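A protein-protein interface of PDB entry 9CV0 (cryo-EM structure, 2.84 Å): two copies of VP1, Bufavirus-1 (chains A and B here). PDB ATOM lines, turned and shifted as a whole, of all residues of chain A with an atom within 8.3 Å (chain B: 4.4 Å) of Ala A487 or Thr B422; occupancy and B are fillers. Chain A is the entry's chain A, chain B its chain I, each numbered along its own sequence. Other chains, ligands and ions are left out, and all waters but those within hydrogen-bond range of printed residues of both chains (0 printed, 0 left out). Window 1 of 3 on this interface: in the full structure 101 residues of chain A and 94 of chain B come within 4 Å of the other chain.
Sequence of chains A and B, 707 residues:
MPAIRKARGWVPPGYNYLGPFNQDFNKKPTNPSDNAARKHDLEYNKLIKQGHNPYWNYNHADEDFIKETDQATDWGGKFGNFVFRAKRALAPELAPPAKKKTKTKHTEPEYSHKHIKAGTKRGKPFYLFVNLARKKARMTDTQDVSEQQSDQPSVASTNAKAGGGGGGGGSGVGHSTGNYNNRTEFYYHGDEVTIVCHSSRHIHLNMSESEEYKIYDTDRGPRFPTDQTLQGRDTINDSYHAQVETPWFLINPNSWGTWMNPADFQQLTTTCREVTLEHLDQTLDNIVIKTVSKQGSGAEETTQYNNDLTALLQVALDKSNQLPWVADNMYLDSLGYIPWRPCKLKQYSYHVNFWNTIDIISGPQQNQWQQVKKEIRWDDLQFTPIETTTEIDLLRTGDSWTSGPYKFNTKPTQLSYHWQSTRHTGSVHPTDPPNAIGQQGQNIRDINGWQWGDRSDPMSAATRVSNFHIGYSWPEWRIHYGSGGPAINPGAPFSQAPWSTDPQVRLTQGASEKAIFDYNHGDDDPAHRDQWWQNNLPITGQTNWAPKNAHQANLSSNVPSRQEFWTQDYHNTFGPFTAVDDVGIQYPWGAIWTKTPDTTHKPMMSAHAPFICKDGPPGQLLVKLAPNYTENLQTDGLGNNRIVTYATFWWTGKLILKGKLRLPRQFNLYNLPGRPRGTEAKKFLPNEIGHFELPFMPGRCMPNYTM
Printed residues of chain A that touch a printed residue of chain B: Ile A236, Asp A238, Asp A328, His A351, Phe A354, His A480, Ser A483, Gly A484, Gly A485, Pro A486, Ala A487, Ile A488 and Asn A489. Hydrophobic or aromatic side chains of chain A that line the printed part of chain B: His A351, Phe A354, His A480, Pro A486 and Ala A487. Hydrophobic or aromatic side chains of chain B that line the printed part of chain A: His B424, Ala B462 and His B469. Among the printed residues, Asp or Glu carboxylates within 4 Å of a Lys or Arg side-chain nitrogen of the other chain: Asp A238 with Arg B423 and Asp A328 with Arg B464.
Ala A487 touches just these residues of chain B: Thr B422 and Ala B462. Of chain A, only Ala A487 comes within 4 Å of Thr B422. Ser B421 touches just these residues of chain A: Ser A483 and Gly A484. Of the printed residues of chain B, Pro A486 touches Arg B423 and Ala B462. Of the printed residues of chain B, Ser A483 touches Ser B421 and His B424. Of the printed residues of chain B, Ile A488 touches Ala B462 and His B469. Ile B470 touches none of the printed residues of chain A. Trp A477 touches none of the printed residues of chain B. The nearest residue of chain A that does not touch Thr B422 is His A480 (5.1 Å). The nearest printed residue of chain B that does not touch Asp A238 is Arg B464 (7.4 Å).
Among the printed residues, merely in contact across the chains: Ile A236 with Ala B462 (3.2 Å), His A351 with Arg B423 (3.6 Å), His A351 with His B424 (3.5 Å), His A351 with Thr B425 (3.8 Å), Phe A354 with Arg B423 (3.98 Å), His A480 with His B469 (3.1 Å), Ser A483 with Ser B421 (3.7 Å), Ser A483 with His B424 (3.7 Å), Gly A484 with Arg B423 (3.8 Å), Gly A484 with His B424 (3.4 Å), Gly A485 with Arg B423 (3.6 Å), Pro A486 with Ala B462 (3.2 Å), Ala A487 with Thr B422 (3.5 Å), Ala A487 with Ala B462 (3.5 Å), Ile A488 with Ala B462 (3.6 Å), Ile A488 with His B469 (3.4 Å) and Asn A489 with His B469 (3.7 Å).
No position is printed for both chains. Of the 23 pairs that touch across the chains among the printed residues, none has its exchanged pair printed and touching as well.
The backbone carbonyl oxygen (O) of Asp A238 sits at hydrogen-bond distance from the backbone NH (N) of Ala B462. The side-chain carboxylate (OD2) of Asp A238 is in salt-bridge range of the guanidinium group (NH2) of Arg B423, at 3.7 Å. The backbone NH of Gly A484 sits at hydrogen-bond distance from the side-chain hydroxyl of Ser B421, 3.5 Å away. NE2 of His B424 sits close to O of Phe A354 (3.1 Å). O of Pro A486 is in hydrogen-bond range of NH1 of Arg B423 (2.7 Å). OD2 of Asp A328 lies within salt-bridge range of NH2 of Arg B464 (2.9 Å).
The side-chain hydroxyl of Ser B421 sits close to the backbone NH of Arg B423, at 3.3 Å. O of Arg A478 lies within hydrogen-bond range of N of Asn A489, 2.8 Å away. The backbone NH (N) of His A480 is in hydrogen-bond range of the backbone carbonyl oxygen (O) of Ala A487, 2.7 Å away.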
ATOM      1  N   THR A 235     -29.340   5.125 -11.596  1.00  0.00           N
ATOM      2  CA  THR A 235     -28.924   5.777 -12.869  1.00  0.00           C
ATOM      3  C   THR A 235     -27.470   5.417 -13.189  1.00  0.00           C
ATOM      4  O   THR A 235     -27.006   5.783 -14.284  1.00  0.00           O
ATOM      5  CB  THR A 235     -29.153   7.291 -12.803  1.00  0.00           C
ATOM      6  OG1 THR A 235     -28.521   7.779 -11.621  1.00  0.00           O
ATOM      7  CG2 THR A 235     -30.619   7.664 -12.790  1.00  0.00           C
ATOM      8  N   ILE A 236     -26.781   4.740 -12.267  1.00  0.00           N
ATOM      9  CA  ILE A 236     -25.375   4.299 -12.507  1.00  0.00           C
ATOM     10  C   ILE A 236     -25.406   3.109 -13.470  1.00  0.00           C
ATOM     11  O   ILE A 236     -24.325   2.674 -13.906  1.00  0.00           O
ATOM     12  CB  ILE A 236     -24.687   3.941 -11.175  1.00  0.00           C
ATOM     13  CG1 ILE A 236     -23.171   3.793 -11.336  1.00  0.00           C
ATOM     14  CG2 ILE A 236     -25.314   2.700 -10.560  1.00  0.00           C
ATOM     15  CD1 ILE A 236     -22.454   3.412 -10.064  1.00  0.00           C
ATOM     16  N   ASP A 238     -26.582   3.182 -16.417  1.00  0.00           N
ATOM     17  CA  ASP A 238     -26.723   3.726 -17.759  1.00  0.00           C
ATOM     18  C   ASP A 238     -25.687   3.126 -18.699  1.00  0.00           C
ATOM     19  O   ASP A 238     -24.484   3.204 -18.443  1.00  0.00           O
ATOM     20  CB  ASP A 238     -26.564   5.244 -17.717  1.00  0.00           C
ATOM     21  CG  ASP A 238     -26.694   5.883 -19.076  1.00  0.00           C
ATOM     22  OD1 ASP A 238     -27.044   5.180 -20.035  1.00  0.00           O
ATOM     23  OD2 ASP A 238     -26.415   7.086 -19.199  1.00  0.00           O
ATOM     24  N   ASP A 328      -8.708  -0.754 -26.044  1.00  0.00           N
ATOM     25  CA  ASP A 328      -8.690  -1.041 -24.585  1.00  0.00           C
ATOM     26  C   ASP A 328      -9.294  -2.438 -24.413  1.00  0.00           C
ATOM     27  O   ASP A 328     -10.339  -2.700 -25.035  1.00  0.00           O
ATOM     28  CB  ASP A 328      -9.443   0.032 -23.801  1.00  0.00           C
ATOM     29  CG  ASP A 328     -10.831   0.309 -24.347  1.00  0.00           C
ATOM     30  OD1 ASP A 328     -10.968   0.371 -25.581  1.00  0.00           O
ATOM     31  OD2 ASP A 328     -11.762   0.453 -23.534  1.00  0.00           O
ATOM     32  N   HIS A 351     -17.374   5.591 -30.595  1.00  0.00           N
ATOM     33  CA  HIS A 351     -18.380   6.547 -30.168  1.00  0.00           C
ATOM     34  C   HIS A 351     -18.396   7.760 -31.078  1.00  0.00           C
ATOM     35  O   HIS A 351     -17.371   8.169 -31.622  1.00  0.00           O
ATOM     36  CB  HIS A 351     -18.113   7.014 -28.739  1.00  0.00           C
ATOM     37  CG  HIS A 351     -18.174   5.928 -27.715  1.00  0.00           C
ATOM     38  ND1 HIS A 351     -19.358   5.388 -27.275  1.00  0.00           N
ATOM     39  CD2 HIS A 351     -17.193   5.281 -27.046  1.00  0.00           C
ATOM     40  CE1 HIS A 351     -19.105   4.462 -26.370  1.00  0.00           C
ATOM     41  NE2 HIS A 351     -17.799   4.378 -26.213  1.00  0.00           N
ATOM     42  N   PHE A 354     -22.338  12.634 -28.508  1.00  0.00           N
ATOM     43  CA  PHE A 354     -23.696  12.593 -28.004  1.00  0.00           C
ATOM     44  C   PHE A 354     -23.709  13.252 -26.639  1.00  0.00           C
ATOM     45  O   PHE A 354     -22.691  13.297 -25.951  1.00  0.00           O
ATOM     46  CB  PHE A 354     -24.241  11.151 -27.923  1.00  0.00           C
ATOM     47  CG  PHE A 354     -23.474  10.256 -26.995  1.00  0.00           C
ATOM     48  CD1 PHE A 354     -23.847  10.121 -25.677  1.00  0.00           C
ATOM     49  CD2 PHE A 354     -22.372   9.557 -27.441  1.00  0.00           C
ATOM     50  CE1 PHE A 354     -23.146   9.320 -24.834  1.00  0.00           C
ATOM     51  CE2 PHE A 354     -21.666   8.750 -26.593  1.00  0.00           C
ATOM     52  CZ  PHE A 354     -22.054   8.634 -25.289  1.00  0.00           C
ATOM     53  N   TRP A 477     -15.795   5.543  -5.100  1.00  0.00           N
ATOM     54  CA  TRP A 477     -16.997   5.309  -5.941  1.00  0.00           C
ATOM     55  C   TRP A 477     -17.559   6.676  -6.328  1.00  0.00           C
ATOM     56  O   TRP A 477     -18.755   6.911  -6.102  1.00  0.00           O
ATOM     57  CB  TRP A 477     -17.990   4.376  -5.243  1.00  0.00           C
ATOM     58  CG  TRP A 477     -17.375   3.037  -4.975  1.00  0.00           C
ATOM     59  CD1 TRP A 477     -17.583   2.233  -3.893  1.00  0.00           C
ATOM     60  CD2 TRP A 477     -16.403   2.359  -5.794  1.00  0.00           C
ATOM     61  NE1 TRP A 477     -16.826   1.096  -3.990  1.00  0.00           N
ATOM     62  CE2 TRP A 477     -16.092   1.146  -5.144  1.00  0.00           C
ATOM     63  CE3 TRP A 477     -15.775   2.648  -7.010  1.00  0.00           C
ATOM     64  CZ2 TRP A 477     -15.186   0.230  -5.676  1.00  0.00           C
ATOM     65  CZ3 TRP A 477     -14.876   1.744  -7.532  1.00  0.00           C
ATOM     66  CH2 TRP A 477     -14.588   0.551  -6.873  1.00  0.00           C
ATOM     67  N   ARG A 478     -16.691   7.538  -6.862  1.00  0.00           N
ATOM     68  CA  ARG A 478     -17.116   8.882  -7.321  1.00  0.00           C
ATOM     69  C   ARG A 478     -17.804   8.726  -8.675  1.00  0.00           C
ATOM     70  O   ARG A 478     -17.132   8.308  -9.634  1.00  0.00           O
ATOM     71  CB  ARG A 478     -15.901   9.811  -7.414  1.00  0.00           C
ATOM     72  CG  ARG A 478     -16.160  11.127  -8.131  1.00  0.00           C
ATOM     73  CD  ARG A 478     -17.286  11.890  -7.467  1.00  0.00           C
ATOM     74  NE  ARG A 478     -17.053  13.325  -7.457  1.00  0.00           N
ATOM     75  CZ  ARG A 478     -17.877  14.202  -6.904  1.00  0.00           C
ATOM     76  NH1 ARG A 478     -17.592  15.493  -6.932  1.00  0.00           N
ATOM     77  NH2 ARG A 478     -18.986  13.782  -6.324  1.00  0.00           N
ATOM     78  N   ILE A 479     -19.099   9.030  -8.736  1.00  0.00           N
ATOM     79  CA  ILE A 479     -19.856   8.956 -10.019  1.00  0.00           C
ATOM     80  C   ILE A 479     -19.846  10.347 -10.654  1.00  0.00           C
ATOM     81  O   ILE A 479     -20.560  11.229 -10.147  1.00  0.00           O
ATOM     82  CB  ILE A 479     -21.292   8.433  -9.815  1.00  0.00           C
ATOM     83  CG1 ILE A 479     -21.323   7.090  -9.079  1.00  0.00           C
ATOM     84  CG2 ILE A 479     -22.025   8.361 -11.146  1.00  0.00           C
ATOM     85  CD1 ILE A 479     -21.311   7.210  -7.575  1.00  0.00           C
ATOM     86  N   HIS A 480     -19.053  10.531 -11.709  1.00  0.00           N
ATOM     87  CA  HIS A 480     -19.045  11.825 -12.435  1.00  0.00           C
ATOM     88  C   HIS A 480     -20.144  11.808 -13.500  1.00  0.00           C
ATOM     89  O   HIS A 480     -20.030  11.010 -14.446  1.00  0.00           O
ATOM     90  CB  HIS A 480     -17.666  12.092 -13.046  1.00  0.00           C
ATOM     91  CG  HIS A 480     -17.674  13.163 -14.084  1.00  0.00           C
ATOM     92  ND1 HIS A 480     -18.407  14.324 -13.941  1.00  0.00           N
ATOM     93  CD2 HIS A 480     -17.043  13.258 -15.273  1.00  0.00           C
ATOM     94  CE1 HIS A 480     -18.233  15.084 -15.001  1.00  0.00           C
ATOM     95  NE2 HIS A 480     -17.397  14.455 -15.832  1.00  0.00           N
ATOM     96  N   TYR A 481     -21.164  12.653 -13.347  1.00  0.00           N
ATOM     97  CA  TYR A 481     -22.233  12.755 -14.373  1.00  0.00           C
ATOM     98  C   TYR A 481     -21.781  13.745 -15.451  1.00  0.00           C
ATOM     99  O   TYR A 481     -22.082  14.943 -15.317  1.00  0.00           O
ATOM    100  CB  TYR A 481     -23.554  13.155 -13.714  1.00  0.00           C
ATOM    101  CG  TYR A 481     -24.249  12.030 -12.991  1.00  0.00           C
ATOM    102  CD1 TYR A 481     -25.227  11.277 -13.618  1.00  0.00           C
ATOM    103  CD2 TYR A 481     -23.921  11.709 -11.685  1.00  0.00           C
ATOM    104  CE1 TYR A 481     -25.868  10.238 -12.964  1.00  0.00           C
ATOM    105  CE2 TYR A 481     -24.552  10.673 -11.017  1.00  0.00           C
ATOM    106  CZ  TYR A 481     -25.529   9.934 -11.659  1.00  0.00           C
ATOM    107  OH  TYR A 481     -26.154   8.911 -11.008  1.00  0.00           O
ATOM    108  N   GLY A 482     -21.083  13.259 -16.481  1.00  0.00           N
ATOM    109  CA  GLY A 482     -20.531  14.154 -17.515  1.00  0.00           C
ATOM    110  C   GLY A 482     -21.401  14.267 -18.751  1.00  0.00           C
ATOM    111  O   GLY A 482     -22.555  13.807 -18.703  1.00  0.00           O
ATOM    112  N   SER A 483     -20.864  14.866 -19.817  1.00  0.00           N
ATOM    113  CA  SER A 483     -21.639  15.080 -21.069  1.00  0.00           C
ATOM    114  C   SER A 483     -22.107  13.744 -21.647  1.00  0.00           C
ATOM    115  O   SER A 483     -23.198  13.716 -22.236  1.00  0.00           O
ATOM    116  CB  SER A 483     -20.819  15.846 -22.075  1.00  0.00           C
ATOM    117  OG  SER A 483     -19.636  15.139 -22.408  1.00  0.00           O
ATOM    118  N   GLY A 484     -21.306  12.688 -21.495  1.00  0.00           N
ATOM    119  CA  GLY A 484     -21.660  11.410 -22.072  1.00  0.00           C
ATOM    120  C   GLY A 484     -22.464  10.515 -21.176  1.00  0.00           C
ATOM    121  O   GLY A 484     -23.080   9.563 -21.652  1.00  0.00           O
ATOM    122  N   GLY A 485     -22.443  10.771 -19.881  1.00  0.00           N
ATOM    123  CA  GLY A 485     -23.276  10.081 -18.936  1.00  0.00           C
ATOM    124  C   GLY A 485     -22.512   9.912 -17.650  1.00  0.00           C
ATOM    125  O   GLY A 485     -21.386  10.390 -17.520  1.00  0.00           O
ATOM    126  N   PRO A 486     -23.080   9.195 -16.689  1.00  0.00           N
ATOM    127  CA  PRO A 486     -22.341   8.922 -15.457  1.00  0.00           C
ATOM    128  C   PRO A 486     -21.187   7.966 -15.702  1.00  0.00           C
ATOM    129  O   PRO A 486     -21.286   7.032 -16.494  1.00  0.00           O
ATOM    130  CB  PRO A 486     -23.403   8.307 -14.544  1.00  0.00           C
ATOM    131  CG  PRO A 486     -24.395   7.739 -15.467  1.00  0.00           C
ATOM    132  CD  PRO A 486     -24.448   8.664 -16.633  1.00  0.00           C
ATOM    133  N   ALA A 487     -20.073   8.218 -15.026  1.00  0.00           N
ATOM    134  CA  ALA A 487     -18.953   7.297 -15.040  1.00  0.00           C
ATOM    135  C   ALA A 487     -18.330   7.283 -13.656  1.00  0.00           C
ATOM    136  O   ALA A 487     -18.714   8.048 -12.777  1.00  0.00           O
ATOM    137  CB  ALA A 487     -17.926   7.679 -16.102  1.00  0.00           C
ATOM    138  N   ILE A 488     -17.349   6.412 -13.472  1.00  0.00           N
ATOM    139  CA  ILE A 488     -16.637   6.286 -12.208  1.00  0.00           C
ATOM    140  C   ILE A 488     -15.323   7.035 -12.335  1.00  0.00           C
ATOM    141  O   ILE A 488     -14.610   6.887 -13.334  1.00  0.00           O
ATOM    142  CB  ILE A 488     -16.402   4.816 -11.828  1.00  0.00           C
ATOM    143  CG1 ILE A 488     -17.720   4.088 -11.578  1.00  0.00           C
ATOM    144  CG2 ILE A 488     -15.528   4.719 -10.607  1.00  0.00           C
ATOM    145  CD1 ILE A 488     -18.491   4.609 -10.412  1.00  0.00           C
ATOM    146  N   ASN A 489     -15.013   7.850 -11.338  1.00  0.00           N
ATOM    147  CA  ASN A 489     -13.712   8.485 -11.231  1.00  0.00           C
ATOM    148  C   ASN A 489     -12.939   7.669 -10.199  1.00  0.00           C
ATOM    149  O   ASN A 489     -13.272   7.701  -9.010  1.00  0.00           O
ATOM    150  CB  ASN A 489     -13.879   9.950 -10.839  1.00  0.00           C
ATOM    151  CG  ASN A 489     -12.654  10.769 -11.107  1.00  0.00           C
ATOM    152  OD1 ASN A 489     -11.556  10.246 -11.231  1.00  0.00           O
ATOM    153  ND2 ASN A 489     -12.836  12.065 -11.216  1.00  0.00           N
ATOM    154  N   PRO A 490     -11.922   6.905 -10.618  1.00  0.00           N
ATOM    155  CA  PRO A 490     -11.542   5.697  -9.869  1.00  0.00           C
ATOM    156  C   PRO A 490     -11.070   5.850  -8.427  1.00  0.00           C
ATOM    157  O   PRO A 490     -11.617   5.188  -7.540  1.00  0.00           O
ATOM    158  CB  PRO A 490     -10.407   5.129 -10.722  1.00  0.00           C
ATOM    159  CG  PRO A 490     -10.670   5.631 -12.067  1.00  0.00           C
ATOM    160  CD  PRO A 490     -11.207   6.996 -11.896  1.00  0.00           C
ATOM    161  N   SER B 421     -15.814  12.793 -23.462  1.00  0.00           N
ATOM    162  CA  SER B 421     -15.673  12.535 -22.042  1.00  0.00           C
ATOM    163  C   SER B 421     -15.107  11.134 -21.862  1.00  0.00           C
ATOM    164  O   SER B 421     -14.642  10.500 -22.809  1.00  0.00           O
ATOM    165  CB  SER B 421     -17.001  12.708 -21.319  1.00  0.00           C
ATOM    166  OG  SER B 421     -17.951  11.756 -21.723  1.00  0.00           O
ATOM    167  N   THR B 422     -15.120  10.640 -20.634  1.00  0.00           N
ATOM    168  CA  THR B 422     -14.689   9.276 -20.398  1.00  0.00           C
ATOM    169  C   THR B 422     -15.730   8.255 -20.848  1.00  0.00           C
ATOM    170  O   THR B 422     -15.406   7.070 -20.951  1.00  0.00           O
ATOM    171  CB  THR B 422     -14.337   9.123 -18.918  1.00  0.00           C
ATOM    172  OG1 THR B 422     -13.790   7.827 -18.668  1.00  0.00           O
ATOM    173  CG2 THR B 422     -15.552   9.326 -18.076  1.00  0.00           C
ATOM    174  N   ARG B 423     -16.954   8.689 -21.138  1.00  0.00           N
ATOM    175  CA  ARG B 423     -17.986   7.863 -21.749  1.00  0.00           C
ATOM    176  C   ARG B 423     -17.958   7.890 -23.271  1.00  0.00           C
ATOM    177  O   ARG B 423     -18.658   7.098 -23.902  1.00  0.00           O
ATOM    178  CB  ARG B 423     -19.363   8.303 -21.257  1.00  0.00           C
ATOM    179  CG  ARG B 423     -19.671   7.952 -19.824  1.00  0.00           C
ATOM    180  CD  ARG B 423     -19.938   6.481 -19.680  1.00  0.00           C
ATOM    181  NE  ARG B 423     -21.112   6.087 -20.443  1.00  0.00           N
ATOM    182  CZ  ARG B 423     -22.353   6.112 -19.979  1.00  0.00           C
ATOM    183  NH1 ARG B 423     -22.591   6.482 -18.740  1.00  0.00           N
ATOM    184  NH2 ARG B 423     -23.355   5.746 -20.750  1.00  0.00           N
ATOM    185  N   HIS B 424     -17.193   8.797 -23.870  1.00  0.00           N
ATOM    186  CA  HIS B 424     -17.013   8.889 -25.313  1.00  0.00           C
ATOM    187  C   HIS B 424     -15.741   8.217 -25.792  1.00  0.00           C
ATOM    188  O   HIS B 424     -15.421   8.299 -26.979  1.00  0.00           O
ATOM    189  CB  HIS B 424     -16.976  10.349 -25.749  1.00  0.00           C
ATOM    190  CG  HIS B 424     -18.253  11.087 -25.537  1.00  0.00           C
ATOM    191  ND1 HIS B 424     -19.313  10.991 -26.404  1.00  0.00           N
ATOM    192  CD2 HIS B 424     -18.646  11.924 -24.555  1.00  0.00           C
ATOM    193  CE1 HIS B 424     -20.298  11.751 -25.972  1.00  0.00           C
ATOM    194  NE2 HIS B 424     -19.922  12.321 -24.847  1.00  0.00           N
ATOM    195  N   THR B 425     -15.003   7.573 -24.903  1.00  0.00           N
ATOM    196  CA  THR B 425     -13.573   7.404 -25.095  1.00  0.00           C
ATOM    197  C   THR B 425     -13.137   6.065 -25.677  1.00  0.00           C
ATOM    198  O   THR B 425     -12.592   6.018 -26.782  1.00  0.00           O
ATOM    199  CB  THR B 425     -12.882   7.654 -23.759  1.00  0.00           C
ATOM    200  OG1 THR B 425     -12.979   9.045 -23.438  1.00  0.00           O
ATOM    201  CG2 THR B 425     -11.460   7.261 -23.811  1.00  0.00           C
ATOM    202  N   ALA B 462     -21.352   2.650 -17.679  1.00  0.00           N
ATOM    203  CA  ALA B 462     -20.971   3.645 -16.688  1.00  0.00           C
ATOM    204  C   ALA B 462     -19.867   3.124 -15.780  1.00  0.00           C
ATOM    205  O   ALA B 462     -18.941   3.859 -15.426  1.00  0.00           O
ATOM    206  CB  ALA B 462     -22.189   4.053 -15.870  1.00  0.00           C
ATOM    207  N   ARG B 464     -17.788   0.580 -16.522  1.00  0.00           N
ATOM    208  CA  ARG B 464     -16.629   0.046 -17.222  1.00  0.00           C
ATOM    209  C   ARG B 464     -15.359   0.706 -16.713  1.00  0.00           C
ATOM    210  O   ARG B 464     -15.270   1.932 -16.659  1.00  0.00           O
ATOM    211  CB  ARG B 464     -16.746   0.286 -18.725  1.00  0.00           C
ATOM    212  CG  ARG B 464     -15.542  -0.235 -19.478  1.00  0.00           C
ATOM    213  CD  ARG B 464     -15.595   0.051 -20.939  1.00  0.00           C
ATOM    214  NE  ARG B 464     -15.486   1.474 -21.225  1.00  0.00           N
ATOM    215  CZ  ARG B 464     -14.343   2.125 -21.375  1.00  0.00           C
ATOM    216  NH1 ARG B 464     -14.343   3.414 -21.636  1.00  0.00           N
ATOM    217  NH2 ARG B 464     -13.198   1.490 -21.274  1.00  0.00           N
ATOM    218  N   SER B 466     -11.816   2.268 -16.931  1.00  0.00           N
ATOM    219  CA  SER B 466     -11.016   2.962 -17.918  1.00  0.00           C
ATOM    220  C   SER B 466      -9.671   3.301 -17.298  1.00  0.00           C
ATOM    221  O   SER B 466      -9.496   3.260 -16.082  1.00  0.00           O
ATOM    222  CB  SER B 466     -11.729   4.216 -18.424  1.00  0.00           C
ATOM    223  OG  SER B 466     -11.972   5.115 -17.366  1.00  0.00           O
ATOM    224  N   PHE B 468      -7.986   6.278 -17.667  1.00  0.00           N
ATOM    225  CA  PHE B 468      -7.853   7.660 -17.258  1.00  0.00           C
ATOM    226  C   PHE B 468      -9.240   8.196 -16.964  1.00  0.00           C
ATOM    227  O   PHE B 468     -10.228   7.466 -16.998  1.00  0.00           O
ATOM    228  CB  PHE B 468      -7.152   8.479 -18.341  1.00  0.00           C
ATOM    229  CG  PHE B 468      -5.909   7.823 -18.864  1.00  0.00           C
ATOM    230  CD1 PHE B 468      -4.779   7.716 -18.082  1.00  0.00           C
ATOM    231  CD2 PHE B 468      -5.863   7.333 -20.149  1.00  0.00           C
ATOM    232  CE1 PHE B 468      -3.645   7.118 -18.565  1.00  0.00           C
ATOM    233  CE2 PHE B 468      -4.725   6.740 -20.627  1.00  0.00           C
ATOM    234  CZ  PHE B 468      -3.618   6.634 -19.833  1.00  0.00           C
ATOM    235  N   HIS B 469      -9.310   9.477 -16.646  1.00  0.00           N
ATOM    236  CA  HIS B 469     -10.589  10.149 -16.517  1.00  0.00           C
ATOM    237  C   HIS B 469     -10.441  11.557 -17.052  1.00  0.00           C
ATOM    238  O   HIS B 469      -9.434  12.216 -16.807  1.00  0.00           O
ATOM    239  CB  HIS B 469     -11.080  10.166 -15.077  1.00  0.00           C
ATOM    240  CG  HIS B 469     -12.529  10.511 -14.945  1.00  0.00           C
ATOM    241  ND1 HIS B 469     -12.984  11.807 -14.861  1.00  0.00           N
ATOM    242  CD2 HIS B 469     -13.627   9.724 -14.916  1.00  0.00           C
ATOM    243  CE1 HIS B 469     -14.301  11.801 -14.766  1.00  0.00           C
ATOM    244  NE2 HIS B 469     -14.715  10.549 -14.798  1.00  0.00           N
ATOM    245  N   ILE B 470     -11.437  12.009 -17.798  1.00  0.00           N
ATOM    246  CA  ILE B 470     -11.377  13.286 -18.491  1.00  0.00           C
ATOM    247  C   ILE B 470     -12.166  14.304 -17.682  1.00  0.00           C
ATOM    248  O   ILE B 470     -13.385  14.185 -17.532  1.00  0.00           O
ATOM    249  CB  ILE B 470     -11.895  13.165 -19.931  1.00  0.00           C
ATOM    250  CG1 ILE B 470     -10.939  12.291 -20.737  1.00  0.00           C
ATOM    251  CG2 ILE B 470     -12.003  14.517 -20.576  1.00  0.00           C
ATOM    252  CD1 ILE B 470     -11.453  11.893 -22.055  1.00  0.00           C
